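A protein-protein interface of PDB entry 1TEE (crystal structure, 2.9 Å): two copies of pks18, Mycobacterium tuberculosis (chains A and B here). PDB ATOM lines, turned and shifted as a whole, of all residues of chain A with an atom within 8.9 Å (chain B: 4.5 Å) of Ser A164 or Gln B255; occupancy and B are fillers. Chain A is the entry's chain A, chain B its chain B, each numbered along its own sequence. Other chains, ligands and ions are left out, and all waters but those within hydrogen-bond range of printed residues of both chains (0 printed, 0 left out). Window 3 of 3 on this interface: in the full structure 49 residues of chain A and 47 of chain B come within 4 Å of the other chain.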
ATOM      1  N   ALA A 132      25.360 -20.860 -11.781  1.00  0.00           N
ATOM      2  CA  ALA A 132      25.177 -21.220 -10.367  1.00  0.00           C
ATOM      3  C   ALA A 132      26.460 -21.224  -9.528  1.00  0.00           C
ATOM      4  O   ALA A 132      26.430 -20.979  -8.318  1.00  0.00           O
ATOM      5  CB  ALA A 132      24.490 -22.583 -10.258  1.00  0.00           C
ATOM      6  N   ALA A 133      27.583 -21.512 -10.162  1.00  0.00           N
ATOM      7  CA  ALA A 133      28.840 -21.538  -9.441  1.00  0.00           C
ATOM      8  C   ALA A 133      29.270 -20.133  -9.021  1.00  0.00           C
ATOM      9  O   ALA A 133      30.053 -19.966  -8.088  1.00  0.00           O
ATOM     10  CB  ALA A 133      29.915 -22.171 -10.307  1.00  0.00           C
ATOM     11  N   ILE A 135      27.276 -17.777  -7.824  1.00  0.00           N
ATOM     12  CA  ILE A 135      26.488 -17.279  -6.709  1.00  0.00           C
ATOM     13  C   ILE A 135      26.951 -17.905  -5.399  1.00  0.00           C
ATOM     14  O   ILE A 135      26.580 -19.037  -5.082  1.00  0.00           O
ATOM     15  CB  ILE A 135      25.021 -17.590  -6.929  1.00  0.00           C
ATOM     16  CG1 ILE A 135      24.587 -16.968  -8.247  1.00  0.00           C
ATOM     17  CG2 ILE A 135      24.196 -17.057  -5.779  1.00  0.00           C
ATOM     18  CD1 ILE A 135      23.306 -17.516  -8.784  1.00  0.00           C
ATOM     19  N   GLY A 136      27.744 -17.149  -4.636  1.00  0.00           N
ATOM     20  CA  GLY A 136      28.285 -17.646  -3.383  1.00  0.00           C
ATOM     21  C   GLY A 136      27.580 -17.340  -2.077  1.00  0.00           C
ATOM     22  O   GLY A 136      27.980 -17.857  -1.035  1.00  0.00           O
ATOM     23  N   LEU A 137      26.557 -16.496  -2.112  1.00  0.00           N
ATOM     24  CA  LEU A 137      25.812 -16.169  -0.898  1.00  0.00           C
ATOM     25  C   LEU A 137      24.322 -16.024  -1.167  1.00  0.00           C
ATOM     26  O   LEU A 137      23.913 -15.539  -2.218  1.00  0.00           O
ATOM     27  CB  LEU A 137      26.334 -14.873  -0.262  1.00  0.00           C
ATOM     28  CG  LEU A 137      25.469 -14.244   0.840  1.00  0.00           C
ATOM     29  CD1 LEU A 137      25.419 -15.155   2.038  1.00  0.00           C
ATOM     30  CD2 LEU A 137      26.038 -12.909   1.236  1.00  0.00           C
ATOM     31  N   LEU A 138      23.516 -16.465  -0.210  1.00  0.00           N
ATOM     32  CA  LEU A 138      22.071 -16.357  -0.304  1.00  0.00           C
ATOM     33  C   LEU A 138      21.623 -15.805   1.041  1.00  0.00           C
ATOM     34  O   LEU A 138      21.978 -16.333   2.086  1.00  0.00           O
ATOM     35  CB  LEU A 138      21.440 -17.730  -0.579  1.00  0.00           C
ATOM     36  CG  LEU A 138      19.930 -17.894  -0.348  1.00  0.00           C
ATOM     37  CD1 LEU A 138      19.169 -16.678  -0.808  1.00  0.00           C
ATOM     38  CD2 LEU A 138      19.443 -19.099  -1.086  1.00  0.00           C
ATOM     39  N   VAL A 156      17.874 -23.101  -2.819  1.00  0.00           N
ATOM     40  CA  VAL A 156      19.124 -23.678  -3.312  1.00  0.00           C
ATOM     41  C   VAL A 156      18.855 -24.894  -4.191  1.00  0.00           C
ATOM     42  O   VAL A 156      19.329 -24.979  -5.322  1.00  0.00           O
ATOM     43  CB  VAL A 156      20.062 -24.101  -2.146  1.00  0.00           C
ATOM     44  CG1 VAL A 156      21.263 -24.850  -2.688  1.00  0.00           C
ATOM     45  CG2 VAL A 156      20.524 -22.876  -1.382  1.00  0.00           C
ATOM     46  N   LEU A 161      21.401 -24.404  -7.183  1.00  0.00           N
ATOM     47  CA  LEU A 161      22.541 -23.604  -6.788  1.00  0.00           C
ATOM     48  C   LEU A 161      23.560 -24.582  -6.227  1.00  0.00           C
ATOM     49  O   LEU A 161      23.345 -25.796  -6.284  1.00  0.00           O
ATOM     50  CB  LEU A 161      22.125 -22.583  -5.739  1.00  0.00           C
ATOM     51  CG  LEU A 161      21.066 -21.597  -6.242  1.00  0.00           C
ATOM     52  CD1 LEU A 161      20.625 -20.693  -5.104  1.00  0.00           C
ATOM     53  CD2 LEU A 161      21.631 -20.770  -7.398  1.00  0.00           C
ATOM     54  N   SER A 162      24.667 -24.074  -5.696  1.00  0.00           N
ATOM     55  CA  SER A 162      25.695 -24.951  -5.161  1.00  0.00           C
ATOM     56  C   SER A 162      25.460 -25.444  -3.741  1.00  0.00           C
ATOM     57  O   SER A 162      25.032 -24.695  -2.865  1.00  0.00           O
ATOM     58  CB  SER A 162      27.057 -24.278  -5.211  1.00  0.00           C
ATOM     59  OG  SER A 162      28.024 -25.107  -4.586  1.00  0.00           O
ATOM     60  N   PRO A 163      25.750 -26.730  -3.503  1.00  0.00           N
ATOM     61  CA  PRO A 163      25.594 -27.370  -2.199  1.00  0.00           C
ATOM     62  C   PRO A 163      26.502 -26.667  -1.194  1.00  0.00           C
ATOM     63  O   PRO A 163      26.313 -26.764   0.023  1.00  0.00           O
ATOM     64  CB  PRO A 163      26.060 -28.799  -2.466  1.00  0.00           C
ATOM     65  CG  PRO A 163      25.759 -28.987  -3.910  1.00  0.00           C
ATOM     66  CD  PRO A 163      26.207 -27.704  -4.507  1.00  0.00           C
ATOM     67  N   SER A 164      27.494 -25.959  -1.723  1.00  0.00           N
ATOM     68  CA  SER A 164      28.456 -25.257  -0.893  1.00  0.00           C
ATOM     69  C   SER A 164      28.190 -23.760  -0.735  1.00  0.00           C
ATOM     70  O   SER A 164      28.932 -23.069  -0.039  1.00  0.00           O
ATOM     71  CB  SER A 164      29.852 -25.467  -1.452  1.00  0.00           C
ATOM     72  OG  SER A 164      29.908 -25.012  -2.782  1.00  0.00           O
ATOM     73  N   ILE A 165      27.134 -23.268  -1.375  1.00  0.00           N
ATOM     74  CA  ILE A 165      26.773 -21.863  -1.286  1.00  0.00           C
ATOM     75  C   ILE A 165      26.599 -21.488   0.181  1.00  0.00           C
ATOM     76  O   ILE A 165      26.243 -22.338   0.998  1.00  0.00           O
ATOM     77  CB  ILE A 165      25.444 -21.589  -2.016  1.00  0.00           C
ATOM     78  CG1 ILE A 165      25.245 -20.084  -2.200  1.00  0.00           C
ATOM     79  CG2 ILE A 165      24.275 -22.138  -1.198  1.00  0.00           C
ATOM     80  CD1 ILE A 165      23.931 -19.700  -2.879  1.00  0.00           C
ATOM     81  N   SER A 166      26.848 -20.219   0.500  1.00  0.00           N
ATOM     82  CA  SER A 166      26.709 -19.697   1.862  1.00  0.00           C
ATOM     83  C   SER A 166      25.310 -19.159   2.078  1.00  0.00           C
ATOM     84  O   SER A 166      24.715 -18.556   1.174  1.00  0.00           O
ATOM     85  CB  SER A 166      27.697 -18.567   2.128  1.00  0.00           C
ATOM     86  OG  SER A 166      29.015 -19.065   2.180  1.00  0.00           O
ATOM     87  N   ARG A 167      24.791 -19.365   3.286  1.00  0.00           N
ATOM     88  CA  ARG A 167      23.456 -18.910   3.605  1.00  0.00           C
ATOM     89  C   ARG A 167      23.362 -18.229   4.951  1.00  0.00           C
ATOM     90  O   ARG A 167      23.993 -18.631   5.926  1.00  0.00           O
ATOM     91  CB  ARG A 167      22.492 -20.089   3.516  1.00  0.00           C
ATOM     92  CG  ARG A 167      22.533 -20.711   2.131  1.00  0.00           C
ATOM     93  CD  ARG A 167      21.687 -21.947   1.986  1.00  0.00           C
ATOM     94  NE  ARG A 167      22.240 -23.082   2.714  1.00  0.00           N
ATOM     95  CZ  ARG A 167      21.906 -23.402   3.955  1.00  0.00           C
ATOM     96  NH1 ARG A 167      21.014 -22.679   4.614  1.00  0.00           N
ATOM     97  NH2 ARG A 167      22.473 -24.444   4.534  1.00  0.00           N
ATOM     98  N   TYR A 188      29.884  -9.124   1.515  1.00  0.00           N
ATOM     99  CA  TYR A 188      30.286 -10.354   0.868  1.00  0.00           C
ATOM    100  C   TYR A 188      30.864 -10.074  -0.519  1.00  0.00           C
ATOM    101  O   TYR A 188      31.993 -10.448  -0.831  1.00  0.00           O
ATOM    102  CB  TYR A 188      29.089 -11.324   0.742  1.00  0.00           C
ATOM    103  CG  TYR A 188      29.429 -12.565  -0.062  1.00  0.00           C
ATOM    104  CD1 TYR A 188      30.431 -13.436   0.371  1.00  0.00           C
ATOM    105  CD2 TYR A 188      28.859 -12.794  -1.313  1.00  0.00           C
ATOM    106  CE1 TYR A 188      30.869 -14.490  -0.422  1.00  0.00           C
ATOM    107  CE2 TYR A 188      29.297 -13.854  -2.119  1.00  0.00           C
ATOM    108  CZ  TYR A 188      30.306 -14.690  -1.663  1.00  0.00           C
ATOM    109  OH  TYR A 188      30.798 -15.700  -2.456  1.00  0.00           O
ATOM    110  N   MET A 195      32.400 -13.187  -6.981  1.00  0.00           N
ATOM    111  CA  MET A 195      31.160 -13.882  -6.671  1.00  0.00           C
ATOM    112  C   MET A 195      29.956 -12.954  -6.671  1.00  0.00           C
ATOM    113  O   MET A 195      30.108 -11.730  -6.629  1.00  0.00           O
ATOM    114  CB  MET A 195      31.287 -14.584  -5.318  1.00  0.00           C
ATOM    115  CG  MET A 195      32.457 -15.552  -5.254  1.00  0.00           C
ATOM    116  SD  MET A 195      32.417 -16.746  -6.602  1.00  0.00           S
ATOM    117  CE  MET A 195      31.109 -17.849  -6.029  1.00  0.00           C
ATOM    118  N   SER B 254      30.774 -24.619   3.626  1.00  0.00           N
ATOM    119  CA  SER B 254      29.402 -25.073   3.817  1.00  0.00           C
ATOM    120  C   SER B 254      29.122 -26.234   2.882  1.00  0.00           C
ATOM    121  O   SER B 254      29.739 -26.351   1.832  1.00  0.00           O
ATOM    122  CB  SER B 254      28.406 -23.957   3.497  1.00  0.00           C
ATOM    123  OG  SER B 254      28.675 -22.776   4.230  1.00  0.00           O
ATOM    124  N   GLN B 255      28.186 -27.092   3.268  1.00  0.00           N
ATOM    125  CA  GLN B 255      27.805 -28.235   2.450  1.00  0.00           C
ATOM    126  C   GLN B 255      26.420 -28.718   2.786  1.00  0.00           C
ATOM    127  O   GLN B 255      26.174 -29.206   3.886  1.00  0.00           O
ATOM    128  CB  GLN B 255      28.779 -29.393   2.632  1.00  0.00           C
ATOM    129  CG  GLN B 255      29.752 -29.527   1.487  1.00  0.00           C
ATOM    130  CD  GLN B 255      29.057 -29.550   0.137  1.00  0.00           C
ATOM    131  OE1 GLN B 255      28.229 -30.415  -0.124  1.00  0.00           O
ATOM    132  NE2 GLN B 255      29.390 -28.593  -0.726  1.00  0.00           N
ATOM    133  N   LEU B 256      25.510 -28.561   1.836  1.00  0.00           N
ATOM    134  CA  LEU B 256      24.151 -29.019   2.016  1.00  0.00           C
ATOM    135  C   LEU B 256      24.248 -30.472   1.597  1.00  0.00           C
ATOM    136  O   LEU B 256      24.617 -30.762   0.464  1.00  0.00           O
ATOM    137  CB  LEU B 256      23.207 -28.290   1.071  1.00  0.00           C
ATOM    138  CG  LEU B 256      21.764 -28.080   1.521  1.00  0.00           C
ATOM    139  CD1 LEU B 256      20.882 -28.003   0.294  1.00  0.00           C
ATOM    140  CD2 LEU B 256      21.311 -29.206   2.406  1.00  0.00           C
ATOM    141  N   LEU B 257      23.946 -31.388   2.509  1.00  0.00           N
ATOM    142  CA  LEU B 257      24.020 -32.804   2.195  1.00  0.00           C
ATOM    143  C   LEU B 257      22.741 -33.282   1.500  1.00  0.00           C
ATOM    144  O   LEU B 257      21.630 -33.035   1.979  1.00  0.00           O
ATOM    145  CB  LEU B 257      24.246 -33.604   3.474  1.00  0.00           C
ATOM    146  CG  LEU B 257      25.435 -33.220   4.354  1.00  0.00           C
ATOM    147  CD1 LEU B 257      25.401 -34.062   5.625  1.00  0.00           C
ATOM    148  CD2 LEU B 257      26.743 -33.429   3.606  1.00  0.00           C
ATOM    149  N   VAL B 292      33.556 -33.700   2.734  1.00  0.00           N
ATOM    150  CA  VAL B 292      33.647 -32.242   2.737  1.00  0.00           C
ATOM    151  C   VAL B 292      35.035 -31.836   3.215  1.00  0.00           C
ATOM    152  O   VAL B 292      35.832 -31.295   2.454  1.00  0.00           O
ATOM    153  CB  VAL B 292      32.613 -31.619   3.684  1.00  0.00           C
ATOM    154  CG1 VAL B 292      32.713 -30.104   3.648  1.00  0.00           C
ATOM    155  CG2 VAL B 292      31.229 -32.068   3.296  1.00  0.00           C
ATOM    156  N   VAL B 381      20.591 -30.162   6.891  1.00  0.00           N
ATOM    157  CA  VAL B 381      21.783 -30.938   7.191  1.00  0.00           C
ATOM    158  C   VAL B 381      22.848 -30.358   6.309  1.00  0.00           C
ATOM    159  O   VAL B 381      23.120 -30.802   5.188  1.00  0.00           O
ATOM    160  CB  VAL B 381      21.635 -32.447   6.994  1.00  0.00           C
ATOM    161  CG1 VAL B 381      22.899 -33.125   7.479  1.00  0.00           C
ATOM    162  CG2 VAL B 381      20.462 -32.962   7.804  1.00  0.00           C
ATOM    163  N   THR B 382      23.405 -29.295   6.866  1.00  0.00           N
ATOM    164  CA  THR B 382      24.444 -28.513   6.259  1.00  0.00           C
ATOM    165  C   THR B 382      25.635 -28.591   7.167  1.00  0.00           C
ATOM    166  O   THR B 382      25.533 -28.338   8.373  1.00  0.00           O
ATOM    167  CB  THR B 382      24.015 -27.060   6.171  1.00  0.00           C
ATOM    168  OG1 THR B 382      22.658 -27.010   5.717  1.00  0.00           O
ATOM    169  CG2 THR B 382      24.920 -26.288   5.221  1.00  0.00           C
ATOM    170  N   VAL B 383      26.763 -28.967   6.590  1.00  0.00           N
ATOM    171  CA  VAL B 383      27.985 -29.031   7.351  1.00  0.00           C
ATOM    172  C   VAL B 383      28.619 -27.662   7.162  1.00  0.00           C
ATOM    173  O   VAL B 383      28.843 -27.229   6.036  1.00  0.00           O
ATOM    174  CB  VAL B 383      28.908 -30.120   6.816  1.00  0.00           C
ATOM    175  CG1 VAL B 383      30.179 -30.180   7.644  1.00  0.00           C
ATOM    176  CG2 VAL B 383      28.188 -31.449   6.856  1.00  0.00           C
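Ser B254 touches Pro A163. Gln B255 touches Pro A163. Ser B254 touches Ser A164. Ile A165 touches Ser B254.
Gln B255 touches just these residues of chain A: Pro A163 and Ser A164. Ser B254 touches just these residues of chain A: Pro A163, Ser A164 and Ile A165. Thr B382 touches just one residue of chain A: Arg A167. Printed residues of chain A within 4 Å of Leu B256: Pro A163 (2.7 Å). Of the printed residues of chain B, Arg A167 touches Thr B382 (2.8 Å). Of the printed residues of chain B, Pro A163 touches Ser B254 (3.9 Å), Gln B255 (3.2 Å) and Leu B256 (2.7 Å). Of the printed residues of chain B, Ile A165 touches Ser B254. The nearest printed residue of chain B that does not touch Ser A164 is Leu B256 (4.8 Å). The nearest printed residue of chain B that does not touch Arg A167 is Leu B256 (4.8 Å).
The guanidinium group of Arg A167 sits at hydrogen-bond distance from the side-chain hydroxyl of Thr B382. NE2 of Gln B255 lies close to N of Ser A164 (3.4 Å). O of Pro A163 lies within hydrogen-bond range of N of Leu B256 (2.7 Å).
Of the 8 printed residues of chain B, 4 touch a printed residue of chain A. Hydrophobic or aromatic side chains of chain B that line the printed part of chain A: Leu B256. Printed residues of chain A that touch a printed residue of chain B: Pro A163, Ser A164, Ile A165 and Arg A167. Among the printed residues, no Asp or Glu carboxylate lies within 4 Å of a Lys or Arg side-chain nitrogen of the other chain.
N of Val B383 is in hydrogen-bond range of O of Gln B255 (2.8 Å). The side-chain hydroxyl of Ser A164 is in hydrogen-bond range of the side-chain hydroxyl of Ser A162 (2.6 Å).
No position is printed for both chains.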
